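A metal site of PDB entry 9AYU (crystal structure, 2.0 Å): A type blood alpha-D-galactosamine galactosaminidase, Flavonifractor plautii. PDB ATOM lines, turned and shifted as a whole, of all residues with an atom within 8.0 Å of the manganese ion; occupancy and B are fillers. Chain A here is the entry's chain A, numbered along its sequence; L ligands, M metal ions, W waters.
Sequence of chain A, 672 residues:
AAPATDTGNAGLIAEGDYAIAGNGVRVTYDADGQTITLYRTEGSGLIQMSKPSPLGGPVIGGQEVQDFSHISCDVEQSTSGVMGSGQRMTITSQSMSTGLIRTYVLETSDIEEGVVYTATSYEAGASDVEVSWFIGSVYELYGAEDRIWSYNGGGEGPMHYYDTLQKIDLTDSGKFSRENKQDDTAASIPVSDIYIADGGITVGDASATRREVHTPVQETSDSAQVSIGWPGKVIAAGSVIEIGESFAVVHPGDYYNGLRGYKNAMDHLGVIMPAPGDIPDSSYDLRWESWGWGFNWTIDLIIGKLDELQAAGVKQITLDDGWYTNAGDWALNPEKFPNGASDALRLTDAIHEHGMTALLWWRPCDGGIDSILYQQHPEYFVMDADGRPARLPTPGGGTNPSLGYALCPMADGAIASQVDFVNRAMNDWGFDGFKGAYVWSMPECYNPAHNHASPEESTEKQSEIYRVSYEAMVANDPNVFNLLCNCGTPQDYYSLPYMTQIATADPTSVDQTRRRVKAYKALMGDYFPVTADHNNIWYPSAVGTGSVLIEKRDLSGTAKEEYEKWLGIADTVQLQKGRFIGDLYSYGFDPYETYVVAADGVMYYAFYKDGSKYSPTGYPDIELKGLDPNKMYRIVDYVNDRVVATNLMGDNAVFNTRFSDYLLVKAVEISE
The side-chain carboxylate (OD1) of Asp 169 sits at hydrogen-bond distance from the side-chain hydroxyl (OG1) of Thr 171, 2.5 Å away. N of Glu 219 sits at hydrogen-bond distance from O of Phe 176 (2.8 Å).
Within 4 Å of the manganese ion: Asp 169, Asp 172, Gly 174 and Glu 219.
The manganese ion is bound by the backbone carbonyl oxygen (O) of Asp 169 (2.2 Å). O2 of the ligand is bound to the manganese ion. O of Gly 174 binds the manganese ion (2.3 Å). OD1 of Asp 172 is bound to the manganese ion (2.3 Å). OE1 of Glu 219 binds the manganese ion, 2.4 Å away. Water W1 is bound to the manganese ion, at 2.5 Å. The side-chain carboxylate (OE2) of Glu 219 is bound to the manganese ion. The manganese ion has seven donor atoms within binding distance.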
ATOM      1  N   ASP A 146     -20.645  31.138 -13.095  1.00  0.00           N
ATOM      2  CA  ASP A 146     -21.362  29.997 -12.539  1.00  0.00           C
ATOM      3  C   ASP A 146     -20.481  29.177 -11.596  1.00  0.00           C
ATOM      4  O   ASP A 146     -21.011  28.498 -10.724  1.00  0.00           O
ATOM      5  CB  ASP A 146     -21.977  29.144 -13.640  1.00  0.00           C
ATOM      6  CG  ASP A 146     -20.972  28.579 -14.644  1.00  0.00           C
ATOM      7  OD1 ASP A 146     -19.930  29.248 -14.929  1.00  0.00           O
ATOM      8  OD2 ASP A 146     -21.252  27.497 -15.149  1.00  0.00           O
ATOM      9  N   LYS A 167     -14.220  22.875  -6.470  1.00  0.00           N
ATOM     10  CA  LYS A 167     -15.107  23.733  -7.220  1.00  0.00           C
ATOM     11  C   LYS A 167     -16.078  24.440  -6.285  1.00  0.00           C
ATOM     12  O   LYS A 167     -16.747  23.814  -5.467  1.00  0.00           O
ATOM     13  CB  LYS A 167     -15.858  22.960  -8.297  1.00  0.00           C
ATOM     14  CG  LYS A 167     -16.670  23.854  -9.218  1.00  0.00           C
ATOM     15  CD  LYS A 167     -17.277  23.118 -10.407  1.00  0.00           C
ATOM     16  CE  LYS A 167     -18.353  22.157  -9.995  1.00  0.00           C
ATOM     17  NZ  LYS A 167     -18.982  21.602 -11.193  1.00  0.00           N
ATOM     18  N   ILE A 168     -16.134  25.773  -6.407  1.00  0.00           N
ATOM     19  CA  ILE A 168     -17.112  26.596  -5.749  1.00  0.00           C
ATOM     20  C   ILE A 168     -18.204  26.884  -6.767  1.00  0.00           C
ATOM     21  O   ILE A 168     -18.051  27.672  -7.683  1.00  0.00           O
ATOM     22  CB  ILE A 168     -16.476  27.883  -5.227  1.00  0.00           C
ATOM     23  CG1 ILE A 168     -15.273  27.571  -4.327  1.00  0.00           C
ATOM     24  CG2 ILE A 168     -17.536  28.721  -4.529  1.00  0.00           C
ATOM     25  CD1 ILE A 168     -14.448  28.781  -3.951  1.00  0.00           C
ATOM     26  N   ASP A 169     -19.298  26.145  -6.610  1.00  0.00           N
ATOM     27  CA  ASP A 169     -20.448  26.272  -7.469  1.00  0.00           C
ATOM     28  C   ASP A 169     -21.287  27.435  -6.976  1.00  0.00           C
ATOM     29  O   ASP A 169     -21.679  27.476  -5.833  1.00  0.00           O
ATOM     30  CB  ASP A 169     -21.178  24.937  -7.468  1.00  0.00           C
ATOM     31  CG  ASP A 169     -22.333  24.792  -8.433  1.00  0.00           C
ATOM     32  OD1 ASP A 169     -22.847  25.808  -8.958  1.00  0.00           O
ATOM     33  OD2 ASP A 169     -22.665  23.631  -8.667  1.00  0.00           O
ATOM     34  N   LEU A 170     -21.566  28.386  -7.870  1.00  0.00           N
ATOM     35  CA  LEU A 170     -22.337  29.573  -7.556  1.00  0.00           C
ATOM     36  C   LEU A 170     -23.803  29.383  -7.919  1.00  0.00           C
ATOM     37  O   LEU A 170     -24.586  30.327  -7.723  1.00  0.00           O
ATOM     38  CB  LEU A 170     -21.702  30.754  -8.268  1.00  0.00           C
ATOM     39  CG  LEU A 170     -20.225  30.993  -7.944  1.00  0.00           C
ATOM     40  CD1 LEU A 170     -19.597  32.044  -8.815  1.00  0.00           C
ATOM     41  CD2 LEU A 170     -19.979  31.345  -6.495  1.00  0.00           C
ATOM     42  N   THR A 171     -24.199  28.196  -8.433  1.00  0.00           N
ATOM     43  CA  THR A 171     -25.565  27.945  -8.869  1.00  0.00           C
ATOM     44  C   THR A 171     -26.305  27.029  -7.901  1.00  0.00           C
ATOM     45  O   THR A 171     -27.484  26.808  -8.095  1.00  0.00           O
ATOM     46  CB  THR A 171     -25.586  27.333 -10.273  1.00  0.00           C
ATOM     47  OG1 THR A 171     -25.086  25.993 -10.154  1.00  0.00           O
ATOM     48  CG2 THR A 171     -24.732  28.119 -11.264  1.00  0.00           C
ATOM     49  N   ASP A 172     -25.634  26.471  -6.900  1.00  0.00           N
ATOM     50  CA  ASP A 172     -26.209  25.455  -6.030  1.00  0.00           C
ATOM     51  C   ASP A 172     -26.720  26.135  -4.756  1.00  0.00           C
ATOM     52  O   ASP A 172     -26.791  27.338  -4.677  1.00  0.00           O
ATOM     53  CB  ASP A 172     -25.220  24.318  -5.729  1.00  0.00           C
ATOM     54  CG  ASP A 172     -24.030  24.755  -4.891  1.00  0.00           C
ATOM     55  OD1 ASP A 172     -23.976  25.948  -4.614  1.00  0.00           O
ATOM     56  OD2 ASP A 172     -23.166  23.915  -4.493  1.00  0.00           O
ATOM     57  N   SER A 173     -27.054  25.343  -3.739  1.00  0.00           N
ATOM     58  CA  SER A 173     -27.560  25.835  -2.479  1.00  0.00           C
ATOM     59  C   SER A 173     -26.436  26.100  -1.491  1.00  0.00           C
ATOM     60  O   SER A 173     -26.545  27.026  -0.699  1.00  0.00           O
ATOM     61  CB  SER A 173     -28.549  24.848  -1.926  1.00  0.00           C
ATOM     62  OG  SER A 173     -28.783  25.099  -0.552  1.00  0.00           O
ATOM     63  N   GLY A 174     -25.331  25.359  -1.535  1.00  0.00           N
ATOM     64  CA  GLY A 174     -24.307  25.445  -0.513  1.00  0.00           C
ATOM     65  C   GLY A 174     -23.450  26.704  -0.620  1.00  0.00           C
ATOM     66  O   GLY A 174     -23.429  27.399  -1.641  1.00  0.00           O
ATOM     67  N   LYS A 175     -22.741  27.014   0.461  1.00  0.00           N
ATOM     68  CA  LYS A 175     -21.768  28.087   0.475  1.00  0.00           C
ATOM     69  C   LYS A 175     -20.440  27.500   0.918  1.00  0.00           C
ATOM     70  O   LYS A 175     -20.288  27.133   2.084  1.00  0.00           O
ATOM     71  CB  LYS A 175     -22.120  29.226   1.445  1.00  0.00           C
ATOM     72  CG  LYS A 175     -23.348  30.000   1.085  1.00  0.00           C
ATOM     73  CD  LYS A 175     -23.307  30.752  -0.249  1.00  0.00           C
ATOM     74  CE  LYS A 175     -24.645  31.401  -0.521  1.00  0.00           C
ATOM     75  NZ  LYS A 175     -24.424  32.575  -1.350  1.00  0.00           N
ATOM     76  N   PHE A 176     -19.514  27.441  -0.014  1.00  0.00           N
ATOM     77  CA  PHE A 176     -18.213  26.883   0.258  1.00  0.00           C
ATOM     78  C   PHE A 176     -17.489  27.764   1.297  1.00  0.00           C
ATOM     79  O   PHE A 176     -17.513  28.982   1.195  1.00  0.00           O
ATOM     80  CB  PHE A 176     -17.376  26.845  -1.011  1.00  0.00           C
ATOM     81  CG  PHE A 176     -16.042  26.150  -0.811  1.00  0.00           C
ATOM     82  CD1 PHE A 176     -14.910  26.861  -0.432  1.00  0.00           C
ATOM     83  CD2 PHE A 176     -15.925  24.786  -1.057  1.00  0.00           C
ATOM     84  CE1 PHE A 176     -13.687  26.208  -0.274  1.00  0.00           C
ATOM     85  CE2 PHE A 176     -14.721  24.143  -0.908  1.00  0.00           C
ATOM     86  CZ  PHE A 176     -13.590  24.848  -0.483  1.00  0.00           C
ATOM     87  N   GLU A 219     -16.983  31.300  -0.332  1.00  0.00           N
ATOM     88  CA  GLU A 219     -17.953  31.722  -1.318  1.00  0.00           C
ATOM     89  C   GLU A 219     -18.675  32.947  -0.788  1.00  0.00           C
ATOM     90  O   GLU A 219     -18.966  33.003   0.406  1.00  0.00           O
ATOM     91  CB  GLU A 219     -18.915  30.566  -1.594  1.00  0.00           C
ATOM     92  CG  GLU A 219     -19.953  30.862  -2.658  1.00  0.00           C
ATOM     93  CD  GLU A 219     -20.817  29.658  -3.001  1.00  0.00           C
ATOM     94  OE1 GLU A 219     -21.830  29.876  -3.732  1.00  0.00           O
ATOM     95  OE2 GLU A 219     -20.479  28.525  -2.572  1.00  0.00           O
ATOM     96  N   THR A 220     -18.966  33.901  -1.675  1.00  0.00           N
ATOM     97  CA  THR A 220     -19.726  35.089  -1.326  1.00  0.00           C
ATOM     98  C   THR A 220     -21.076  35.040  -2.034  1.00  0.00           C
ATOM     99  O   THR A 220     -21.494  33.993  -2.519  1.00  0.00           O
ATOM    100  CB  THR A 220     -18.890  36.327  -1.682  1.00  0.00           C
ATOM    101  OG1 THR A 220     -18.688  36.292  -3.092  1.00  0.00           O
ATOM    102  CG2 THR A 220     -17.556  36.342  -0.954  1.00  0.00           C
ATOM    103  N   SER A 221     -21.763  36.187  -2.102  1.00  0.00           N
ATOM    104  CA  SER A 221     -23.098  36.224  -2.652  1.00  0.00           C
ATOM    105  C   SER A 221     -23.082  35.839  -4.125  1.00  0.00           C
ATOM    106  O   SER A 221     -24.016  35.193  -4.580  1.00  0.00           O
ATOM    107  CB  SER A 221     -23.743  37.552  -2.407  1.00  0.00           C
ATOM    108  OG  SER A 221     -22.967  38.544  -3.056  1.00  0.00           O
ATOM    109  N   SER A 223     -19.710  35.289  -5.824  1.00  0.00           N
ATOM    110  CA  SER A 223     -18.328  35.030  -6.186  1.00  0.00           C
ATOM    111  C   SER A 223     -17.673  34.248  -5.037  1.00  0.00           C
ATOM    112  O   SER A 223     -18.347  33.483  -4.342  1.00  0.00           O
ATOM    113  CB  SER A 223     -17.631  36.329  -6.511  1.00  0.00           C
ATOM    114  OG  SER A 223     -16.315  36.153  -6.965  1.00  0.00           O
HETATM  115  C1  LIG L   1     -19.843  23.770  -3.165  1.00  0.00           C
HETATM  116  O1  LIG L   1     -19.238  24.414  -4.259  1.00  0.00           O
HETATM  117  C2  LIG L   1     -20.681  24.736  -2.387  1.00  0.00           C
HETATM  118  O2  LIG L   1     -21.491  25.559  -3.204  1.00  0.00           O
HETATM  119 MN    MN M   1     -22.504  27.553  -3.753  1.00  0.00          MN
HETATM  120  O   HOH W   1     -24.521  28.854  -4.493  1.00  0.00           O
